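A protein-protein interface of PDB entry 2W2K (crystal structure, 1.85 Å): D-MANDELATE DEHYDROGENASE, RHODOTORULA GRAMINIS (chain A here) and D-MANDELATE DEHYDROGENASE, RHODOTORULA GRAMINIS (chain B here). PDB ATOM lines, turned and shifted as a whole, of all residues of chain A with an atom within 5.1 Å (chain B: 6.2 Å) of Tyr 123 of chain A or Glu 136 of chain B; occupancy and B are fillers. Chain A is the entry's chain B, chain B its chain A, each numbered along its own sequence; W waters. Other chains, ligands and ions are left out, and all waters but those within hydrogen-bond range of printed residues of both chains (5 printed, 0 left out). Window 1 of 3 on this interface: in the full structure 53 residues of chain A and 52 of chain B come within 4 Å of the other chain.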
ATOM      1  N   ASP A 119      -5.220  21.416 -24.218  1.00  0.00           N
ATOM      2  CA  ASP A 119      -5.107  21.214 -22.749  1.00  0.00           C
ATOM      3  C   ASP A 119      -6.109  22.091 -21.975  1.00  0.00           C
ATOM      4  O   ASP A 119      -6.713  21.632 -20.984  1.00  0.00           O
ATOM      5  CB  ASP A 119      -3.684  21.557 -22.261  1.00  0.00           C
ATOM      6  CG  ASP A 119      -2.660  20.431 -22.498  1.00  0.00           C
ATOM      7  OD1 ASP A 119      -3.060  19.306 -22.896  1.00  0.00           O
ATOM      8  OD2 ASP A 119      -1.437  20.685 -22.282  1.00  0.00           O
ATOM      9  N   LEU A 120      -6.268  23.363 -22.387  1.00  0.00           N
ATOM     10  CA  LEU A 120      -7.218  24.287 -21.696  1.00  0.00           C
ATOM     11  C   LEU A 120      -8.670  23.830 -21.916  1.00  0.00           C
ATOM     12  O   LEU A 120      -9.492  23.899 -20.988  1.00  0.00           O
ATOM     13  CB  LEU A 120      -7.012  25.776 -22.122  1.00  0.00           C
ATOM     14  CG  LEU A 120      -7.623  26.947 -21.292  1.00  0.00           C
ATOM     15  CD1 LEU A 120      -9.097  27.233 -21.623  1.00  0.00           C
ATOM     16  CD2 LEU A 120      -7.434  26.814 -19.747  1.00  0.00           C
ATOM     17  N   ALA A 121      -8.989  23.323 -23.111  1.00  0.00           N
ATOM     18  CA  ALA A 121     -10.325  22.719 -23.326  1.00  0.00           C
ATOM     19  C   ALA A 121     -10.579  21.489 -22.422  1.00  0.00           C
ATOM     20  O   ALA A 121     -11.687  21.327 -21.878  1.00  0.00           O
ATOM     21  CB  ALA A 121     -10.535  22.367 -24.825  1.00  0.00           C
ATOM     22  N   LEU A 122      -9.547  20.651 -22.240  1.00  0.00           N
ATOM     23  CA  LEU A 122      -9.632  19.485 -21.333  1.00  0.00           C
ATOM     24  C   LEU A 122      -9.887  19.916 -19.873  1.00  0.00           C
ATOM     25  O   LEU A 122     -10.688  19.279 -19.165  1.00  0.00           O
ATOM     26  CB  LEU A 122      -8.382  18.569 -21.418  1.00  0.00           C
ATOM     27  CG  LEU A 122      -8.606  17.121 -20.890  1.00  0.00           C
ATOM     28  CD1 LEU A 122      -9.429  16.282 -21.896  1.00  0.00           C
ATOM     29  CD2 LEU A 122      -7.258  16.444 -20.592  1.00  0.00           C
ATOM     30  N   TYR A 123      -9.223  20.996 -19.433  1.00  0.00           N
ATOM     31  CA  TYR A 123      -9.489  21.617 -18.118  1.00  0.00           C
ATOM     32  C   TYR A 123     -10.977  22.031 -17.946  1.00  0.00           C
ATOM     33  O   TYR A 123     -11.610  21.731 -16.907  1.00  0.00           O
ATOM     34  CB  TYR A 123      -8.543  22.833 -17.916  1.00  0.00           C
ATOM     35  CG  TYR A 123      -8.877  23.758 -16.744  1.00  0.00           C
ATOM     36  CD1 TYR A 123      -8.337  23.529 -15.471  1.00  0.00           C
ATOM     37  CD2 TYR A 123      -9.702  24.885 -16.919  1.00  0.00           C
ATOM     38  CE1 TYR A 123      -8.627  24.395 -14.389  1.00  0.00           C
ATOM     39  CE2 TYR A 123     -10.016  25.748 -15.829  1.00  0.00           C
ATOM     40  CZ  TYR A 123      -9.471  25.496 -14.580  1.00  0.00           C
ATOM     41  OH  TYR A 123      -9.750  26.352 -13.508  1.00  0.00           O
ATOM     42  N   LEU A 124     -11.531  22.719 -18.947  1.00  0.00           N
ATOM     43  CA  LEU A 124     -12.960  23.130 -18.892  1.00  0.00           C
ATOM     44  C   LEU A 124     -13.919  21.910 -18.884  1.00  0.00           C
ATOM     45  O   LEU A 124     -14.944  21.931 -18.181  1.00  0.00           O
ATOM     46  CB  LEU A 124     -13.304  24.065 -20.052  1.00  0.00           C
ATOM     47  CG  LEU A 124     -12.541  25.412 -20.174  1.00  0.00           C
ATOM     48  CD1 LEU A 124     -12.959  26.111 -21.460  1.00  0.00           C
ATOM     49  CD2 LEU A 124     -12.820  26.299 -18.921  1.00  0.00           C
ATOM     50  N   ILE A 125     -13.582  20.862 -19.643  1.00  0.00           N
ATOM     51  CA  ILE A 125     -14.371  19.581 -19.649  1.00  0.00           C
ATOM     52  C   ILE A 125     -14.395  18.922 -18.257  1.00  0.00           C
ATOM     53  O   ILE A 125     -15.470  18.533 -17.743  1.00  0.00           O
ATOM     54  CB  ILE A 125     -13.866  18.566 -20.752  1.00  0.00           C
ATOM     55  CG1 ILE A 125     -14.171  19.111 -22.154  1.00  0.00           C
ATOM     56  CG2 ILE A 125     -14.550  17.181 -20.589  1.00  0.00           C
ATOM     57  CD1 ILE A 125     -13.435  18.337 -23.342  1.00  0.00           C
ATOM     58  N   LEU A 126     -13.214  18.811 -17.635  1.00  0.00           N
ATOM     59  CA  LEU A 126     -13.137  18.340 -16.248  1.00  0.00           C
ATOM     60  C   LEU A 126     -13.955  19.249 -15.306  1.00  0.00           C
ATOM     61  O   LEU A 126     -14.745  18.746 -14.501  1.00  0.00           O
ATOM     62  CB  LEU A 126     -11.667  18.196 -15.788  1.00  0.00           C
ATOM     63  CG  LEU A 126     -10.868  17.021 -16.395  1.00  0.00           C
ATOM     64  CD1 LEU A 126      -9.332  17.256 -16.364  1.00  0.00           C
ATOM     65  CD2 LEU A 126     -11.218  15.676 -15.737  1.00  0.00           C
ATOM     66  N   SER A 127     -13.795  20.573 -15.422  1.00  0.00           N
ATOM     67  CA  SER A 127     -14.566  21.517 -14.580  1.00  0.00           C
ATOM     68  C   SER A 127     -16.103  21.347 -14.644  1.00  0.00           C
ATOM     69  O   SER A 127     -16.771  21.335 -13.598  1.00  0.00           O
ATOM     70  CB  SER A 127     -14.160  22.986 -14.862  1.00  0.00           C
ATOM     71  OG  SER A 127     -14.751  23.859 -13.907  1.00  0.00           O
ATOM     72  N   SER A 133     -15.472  24.596 -10.287  1.00  0.00           N
ATOM     73  CA  SER A 133     -15.507  26.058 -10.183  1.00  0.00           C
ATOM     74  C   SER A 133     -16.277  26.507  -8.920  1.00  0.00           C
ATOM     75  O   SER A 133     -15.815  27.387  -8.170  1.00  0.00           O
ATOM     76  CB  SER A 133     -16.085  26.684 -11.460  1.00  0.00           C
ATOM     77  OG  SER A 133     -16.028  28.103 -11.382  1.00  0.00           O
ATOM     78  N   GLU A 136     -14.220  25.585  -5.757  1.00  0.00           N
ATOM     79  CA  GLU A 136     -13.169  26.588  -5.461  1.00  0.00           C
ATOM     80  C   GLU A 136     -13.747  27.795  -4.692  1.00  0.00           C
ATOM     81  O   GLU A 136     -13.185  28.233  -3.673  1.00  0.00           O
ATOM     82  CB  GLU A 136     -12.430  27.064  -6.737  1.00  0.00           C
ATOM     83  CG  GLU A 136     -11.557  26.002  -7.441  1.00  0.00           C
ATOM     84  CD  GLU A 136     -10.425  26.600  -8.335  1.00  0.00           C
ATOM     85  OE1 GLU A 136      -9.935  27.717  -8.048  1.00  0.00           O
ATOM     86  OE2 GLU A 136      -9.997  25.936  -9.312  1.00  0.00           O
ATOM     87  N   THR A 300     -18.001  28.157 -15.514  1.00  0.00           N
ATOM     88  CA  THR A 300     -16.542  28.319 -15.442  1.00  0.00           C
ATOM     89  C   THR A 300     -16.122  29.390 -16.470  1.00  0.00           C
ATOM     90  O   THR A 300     -16.453  29.294 -17.667  1.00  0.00           O
ATOM     91  CB  THR A 300     -15.777  26.957 -15.718  1.00  0.00           C
ATOM     92  OG1 THR A 300     -16.210  25.924 -14.810  1.00  0.00           O
ATOM     93  CG2 THR A 300     -14.245  27.139 -15.632  1.00  0.00           C
ATOM     94  N   LEU A 301     -15.416  30.421 -15.993  1.00  0.00           N
ATOM     95  CA  LEU A 301     -15.032  31.576 -16.833  1.00  0.00           C
ATOM     96  C   LEU A 301     -13.529  31.908 -16.726  1.00  0.00           C
ATOM     97  O   LEU A 301     -13.020  32.141 -15.627  1.00  0.00           O
ATOM     98  CB  LEU A 301     -15.881  32.820 -16.466  1.00  0.00           C
ATOM     99  CG  LEU A 301     -17.418  32.650 -16.576  1.00  0.00           C
ATOM    100  CD1 LEU A 301     -18.192  33.587 -15.628  1.00  0.00           C
ATOM    101  CD2 LEU A 301     -17.881  32.773 -18.017  1.00  0.00           C
ATOM    102  N   THR A 302     -12.822  31.922 -17.860  1.00  0.00           N
ATOM    103  CA  THR A 302     -11.365  32.256 -17.898  1.00  0.00           C
ATOM    104  C   THR A 302     -11.056  33.458 -18.853  1.00  0.00           C
ATOM    105  O   THR A 302     -11.861  33.777 -19.745  1.00  0.00           O
ATOM    106  CB  THR A 302     -10.476  30.992 -18.198  1.00  0.00           C
ATOM    107  OG1 THR A 302     -10.955  30.300 -19.374  1.00  0.00           O
ATOM    108  CG2 THR A 302     -10.506  30.013 -17.013  1.00  0.00           C
ATOM    109  N   TYR B 123      -6.871  17.647 -13.186  1.00  0.00           N
ATOM    110  CA  TYR B 123      -7.379  19.046 -13.106  1.00  0.00           C
ATOM    111  C   TYR B 123      -6.419  19.991 -12.337  1.00  0.00           C
ATOM    112  O   TYR B 123      -6.103  21.094 -12.822  1.00  0.00           O
ATOM    113  CB  TYR B 123      -8.792  19.054 -12.474  1.00  0.00           C
ATOM    114  CG  TYR B 123      -9.357  20.411 -12.069  1.00  0.00           C
ATOM    115  CD1 TYR B 123     -10.127  21.165 -12.971  1.00  0.00           C
ATOM    116  CD2 TYR B 123      -9.160  20.925 -10.771  1.00  0.00           C
ATOM    117  CE1 TYR B 123     -10.674  22.415 -12.597  1.00  0.00           C
ATOM    118  CE2 TYR B 123      -9.697  22.158 -10.398  1.00  0.00           C
ATOM    119  CZ  TYR B 123     -10.451  22.897 -11.305  1.00  0.00           C
ATOM    120  OH  TYR B 123     -11.007  24.118 -10.940  1.00  0.00           O
ATOM    121  N   LEU B 126      -3.128  20.537 -14.418  1.00  0.00           N
ATOM    122  CA  LEU B 126      -3.451  21.578 -15.411  1.00  0.00           C
ATOM    123  C   LEU B 126      -3.509  22.996 -14.807  1.00  0.00           C
ATOM    124  O   LEU B 126      -2.870  23.908 -15.339  1.00  0.00           O
ATOM    125  CB  LEU B 126      -4.739  21.230 -16.209  1.00  0.00           C
ATOM    126  CG  LEU B 126      -4.592  20.043 -17.199  1.00  0.00           C
ATOM    127  CD1 LEU B 126      -5.975  19.373 -17.485  1.00  0.00           C
ATOM    128  CD2 LEU B 126      -3.911  20.432 -18.530  1.00  0.00           C
ATOM    129  N   SER B 127      -4.230  23.161 -13.689  1.00  0.00           N
ATOM    130  CA  SER B 127      -4.387  24.454 -12.977  1.00  0.00           C
ATOM    131  C   SER B 127      -3.052  25.100 -12.560  1.00  0.00           C
ATOM    132  O   SER B 127      -2.852  26.315 -12.789  1.00  0.00           O
ATOM    133  CB  SER B 127      -5.338  24.323 -11.751  1.00  0.00           C
ATOM    134  OG  SER B 127      -5.738  25.621 -11.235  1.00  0.00           O
ATOM    135  N   LEU B 131      -1.911  28.465 -14.472  1.00  0.00           N
ATOM    136  CA  LEU B 131      -2.403  29.549 -13.575  1.00  0.00           C
ATOM    137  C   LEU B 131      -3.890  29.867 -13.783  1.00  0.00           C
ATOM    138  O   LEU B 131      -4.305  31.029 -13.819  1.00  0.00           O
ATOM    139  CB  LEU B 131      -1.489  30.815 -13.688  1.00  0.00           C
ATOM    140  CG  LEU B 131       0.020  30.511 -13.527  1.00  0.00           C
ATOM    141  CD1 LEU B 131       0.861  31.779 -13.647  1.00  0.00           C
ATOM    142  CD2 LEU B 131       0.346  29.795 -12.189  1.00  0.00           C
ATOM    143  N   ALA B 132      -4.705  28.816 -13.914  1.00  0.00           N
ATOM    144  CA  ALA B 132      -6.117  28.983 -14.280  1.00  0.00           C
ATOM    145  C   ALA B 132      -7.002  29.498 -13.143  1.00  0.00           C
ATOM    146  O   ALA B 132      -8.020  30.105 -13.399  1.00  0.00           O
ATOM    147  CB  ALA B 132      -6.682  27.684 -14.836  1.00  0.00           C
ATOM    148  N   SER B 133      -6.633  29.189 -11.903  1.00  0.00           N
ATOM    149  CA  SER B 133      -7.358  29.646 -10.707  1.00  0.00           C
ATOM    150  C   SER B 133      -7.351  31.190 -10.622  1.00  0.00           C
ATOM    151  O   SER B 133      -8.383  31.815 -10.402  1.00  0.00           O
ATOM    152  CB  SER B 133      -6.707  29.009  -9.472  1.00  0.00           C
ATOM    153  OG  SER B 133      -7.441  29.225  -8.279  1.00  0.00           O
ATOM    154  N   TYR B 134      -6.181  31.796 -10.824  1.00  0.00           N
ATOM    155  CA  TYR B 134      -6.024  33.266 -10.853  1.00  0.00           C
ATOM    156  C   TYR B 134      -6.812  33.902 -12.006  1.00  0.00           C
ATOM    157  O   TYR B 134      -7.501  34.922 -11.813  1.00  0.00           O
ATOM    158  CB  TYR B 134      -4.521  33.614 -10.911  1.00  0.00           C
ATOM    159  CG  TYR B 134      -4.143  35.099 -10.876  1.00  0.00           C
ATOM    160  CD1 TYR B 134      -4.479  35.917  -9.769  1.00  0.00           C
ATOM    161  CD2 TYR B 134      -3.395  35.666 -11.901  1.00  0.00           C
ATOM    162  CE1 TYR B 134      -4.102  37.286  -9.722  1.00  0.00           C
ATOM    163  CE2 TYR B 134      -2.998  37.032 -11.854  1.00  0.00           C
ATOM    164  CZ  TYR B 134      -3.364  37.827 -10.765  1.00  0.00           C
ATOM    165  OH  TYR B 134      -2.984  39.154 -10.737  1.00  0.00           O
ATOM    166  N   SER B 135      -6.752  33.275 -13.188  1.00  0.00           N
ATOM    167  CA  SER B 135      -7.529  33.707 -14.369  1.00  0.00           C
ATOM    168  C   SER B 135      -9.044  33.722 -14.058  1.00  0.00           C
ATOM    169  O   SER B 135      -9.742  34.681 -14.412  1.00  0.00           O
ATOM    170  CB  SER B 135      -7.219  32.817 -15.598  1.00  0.00           C
ATOM    171  OG  SER B 135      -7.851  33.294 -16.789  1.00  0.00           O
ATOM    172  N   GLU B 136      -9.555  32.674 -13.411  1.00  0.00           N
ATOM    173  CA  GLU B 136     -11.007  32.640 -13.087  1.00  0.00           C
ATOM    174  C   GLU B 136     -11.435  33.815 -12.183  1.00  0.00           C
ATOM    175  O   GLU B 136     -12.469  34.490 -12.423  1.00  0.00           O
ATOM    176  CB  GLU B 136     -11.440  31.293 -12.458  1.00  0.00           C
ATOM    177  CG  GLU B 136     -11.384  30.028 -13.370  1.00  0.00           C
ATOM    178  CD  GLU B 136     -12.259  28.847 -12.837  1.00  0.00           C
ATOM    179  OE1 GLU B 136     -13.328  29.089 -12.213  1.00  0.00           O
ATOM    180  OE2 GLU B 136     -11.892  27.676 -13.069  1.00  0.00           O
ATOM    181  N   ARG B 137     -10.641  34.094 -11.150  1.00  0.00           N
ATOM    182  CA  ARG B 137     -10.962  35.227 -10.273  1.00  0.00           C
ATOM    183  C   ARG B 137     -10.955  36.586 -10.984  1.00  0.00           C
ATOM    184  O   ARG B 137     -11.788  37.437 -10.690  1.00  0.00           O
ATOM    185  CB  ARG B 137     -10.076  35.236  -9.017  1.00  0.00           C
ATOM    186  CG  ARG B 137     -10.247  33.961  -8.244  1.00  0.00           C
ATOM    187  CD  ARG B 137      -9.835  34.051  -6.801  1.00  0.00           C
ATOM    188  NE  ARG B 137      -8.458  34.472  -6.574  1.00  0.00           N
ATOM    189  CZ  ARG B 137      -7.378  33.701  -6.702  1.00  0.00           C
ATOM    190  NH1 ARG B 137      -7.467  32.437  -7.091  1.00  0.00           N
ATOM    191  NH2 ARG B 137      -6.189  34.212  -6.434  1.00  0.00           N
ATOM    192  N   ALA B 138     -10.041  36.767 -11.940  1.00  0.00           N
ATOM    193  CA  ALA B 138     -10.002  37.963 -12.791  1.00  0.00           C
ATOM    194  C   ALA B 138     -11.221  38.084 -13.701  1.00  0.00           C
ATOM    195  O   ALA B 138     -11.827  39.169 -13.830  1.00  0.00           O
ATOM    196  CB  ALA B 138      -8.702  37.977 -13.622  1.00  0.00           C
ATOM    197  N   ALA B 139     -11.603  36.973 -14.337  1.00  0.00           N
ATOM    198  CA  ALA B 139     -12.793  36.987 -15.183  1.00  0.00           C
ATOM    199  C   ALA B 139     -14.052  37.393 -14.383  1.00  0.00           C
ATOM    200  O   ALA B 139     -14.898  38.136 -14.886  1.00  0.00           O
ATOM    201  CB  ALA B 139     -12.986  35.600 -15.895  1.00  0.00           C
ATOM    202  N   ARG B 140     -14.146  36.903 -13.145  1.00  0.00           N
ATOM    203  CA  ARG B 140     -15.336  37.085 -12.285  1.00  0.00           C
ATOM    204  C   ARG B 140     -15.482  38.495 -11.679  1.00  0.00           C
ATOM    205  O   ARG B 140     -16.520  38.804 -11.072  1.00  0.00           O
ATOM    206  CB  ARG B 140     -15.374  36.020 -11.184  1.00  0.00           C
ATOM    207  CG  ARG B 140     -15.525  34.584 -11.745  1.00  0.00           C
ATOM    208  CD  ARG B 140     -15.703  33.553 -10.654  1.00  0.00           C
ATOM    209  NE  ARG B 140     -17.078  33.588 -10.186  1.00  0.00           N
ATOM    210  CZ  ARG B 140     -18.089  32.970 -10.783  1.00  0.00           C
ATOM    211  NH1 ARG B 140     -17.894  32.223 -11.872  1.00  0.00           N
ATOM    212  NH2 ARG B 140     -19.295  33.087 -10.271  1.00  0.00           N
ATOM    213  N   THR B 141     -14.471  39.351 -11.861  1.00  0.00           N
ATOM    214  CA  THR B 141     -14.642  40.794 -11.569  1.00  0.00           C
ATOM    215  C   THR B 141     -15.603  41.499 -12.534  1.00  0.00           C
ATOM    216  O   THR B 141     -16.184  42.525 -12.176  1.00  0.00           O
ATOM    217  CB  THR B 141     -13.303  41.592 -11.556  1.00  0.00           C
ATOM    218  OG1 THR B 141     -12.749  41.653 -12.883  1.00  0.00           O
ATOM    219  CG2 THR B 141     -12.296  40.980 -10.591  1.00  0.00           C
HETATM  220  O   HOH W   1     -12.989  25.394 -12.467  1.00  0.00           O
HETATM  221  O   HOH W   2     -14.339  29.873  -9.249  1.00  0.00           O
HETATM  222  O   HOH W   3     -14.849  31.164 -13.206  1.00  0.00           O
HETATM  223  O   HOH W   4      -8.264  26.302 -11.190  1.00  0.00           O
HETATM  224  O   HOH W   5     -10.379  30.762  -8.356  1.00  0.00           O
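OH of Tyr 123 of chain B sits at hydrogen-bond distance from OE2 of Glu 136 of chain A.
OE1 of Glu 136 of chain A is in hydrogen-bond range of OG of Ser 133 of chain B (2.9 Å).
OH of Tyr 123 of chain A is in hydrogen-bond range of OE2 of Glu 136 of chain B (2.6 Å).
The side-chain hydroxyl (OG) of Ser 133 of chain A sits at hydrogen-bond distance from the side-chain carboxylate (OE1) of Glu 136 of chain B (3.0 Å).
The backbone carbonyl oxygen (O) of Ser 127 of chain B sits at hydrogen-bond distance from the backbone NH (N) of Ala 132 of chain B, 3.3 Å away.
NH1 of Arg 137 of chain B is in hydrogen-bond range of OG of Ser 133 of chain B (3.4 Å).
OG of Ser 127 of chain A sits at hydrogen-bond distance from OG1 of Thr 300 of chain A, at 2.7 Å.
Among the printed residues, pairs that only touch across the chains: Asp 119 of chain A with Leu 126 of chain B, Tyr 123 of chain A with Tyr 123 of chain B, Tyr 123 of chain A with Ala 132 of chain B, Thr 300 of chain A with Glu 136 of chain B, Leu 301 of chain A with Glu 136 of chain B, Leu 301 of chain A with Ala 139 of chain B, Thr 302 of chain A with Ser 135 of chain B and Thr 302 of chain A with Glu 136 of chain B.
Of chain B, only Tyr 123 (3.4 Å), Ala 132 (3.6 Å) and Glu 136 (2.6 Å) come within 4 Å of Tyr 123 of chain A.
Glu 136 of chain B touches just these residues of chain A: Tyr 123, Ser 133, Thr 300, Leu 301 and Thr 302.
Printed residues of chain B within 4 Å of Thr 300 of chain A: Glu 136 (3.5 Å).
Of the printed residues of chain B, Ser 133 of chain A touches Glu 136 (3.0 Å).
Of the printed residues of chain A, Tyr 123 of chain B touches Tyr 123 (3.4 Å) and Glu 136 (2.6 Å).
Ala 121 of chain A touches none of the printed residues of chain B.
Leu 120 of chain A touches none of the printed residues of chain B.
Hydrophobic or aromatic side chains of chain B within 4 Å of the printed part of chain A: Tyr 123, Leu 126, Ala 132 and Ala 139.
Printed residues of chain A that touch a printed residue of chain B: Asp 119, Tyr 123, Ser 133, Glu 136, Thr 300, Leu 301 and Thr 302.
Hydrophobic or aromatic side chains of chain A that line the printed part of chain B: Tyr 123.
Among the printed residues, 12 pairs touch across the chains.
Among the printed residues, no Asp or Glu carboxylate lies within 4 Å of a Lys or Arg side-chain nitrogen of the other chain.
Water W4 lies within hydrogen-bond range of OE2 of Glu 136 of chain A (2.6 Å), OG of Ser 127 of chain B (2.6 Å), OH of Tyr 123 of chain A (2.8 Å) and N of Ser 133 of chain B (3.4 Å).
Water W1 lies within hydrogen-bond range of OE2 of Glu 136 of chain B, OG of Ser 127 of chain A, OH of Tyr 123 of chain B and N of Ser 133 of chain A.
Water W3 lies within hydrogen-bond range of the side-chain carboxylate of Glu 136 of chain B (2.8 Å), the backbone NH of Leu 301 of chain A (2.9 Å) and the guanidinium group of Arg 140 of chain B (3.5 Å).
Water W5 bridges O of Ser 133 of chain B and OE1 of Glu 136 of chain A.
Water W2 lies within hydrogen-bond range of the backbone carbonyl oxygen (O) of Ser 133 of chain A and the side-chain carboxylate (OE1) of Glu 136 of chain B.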
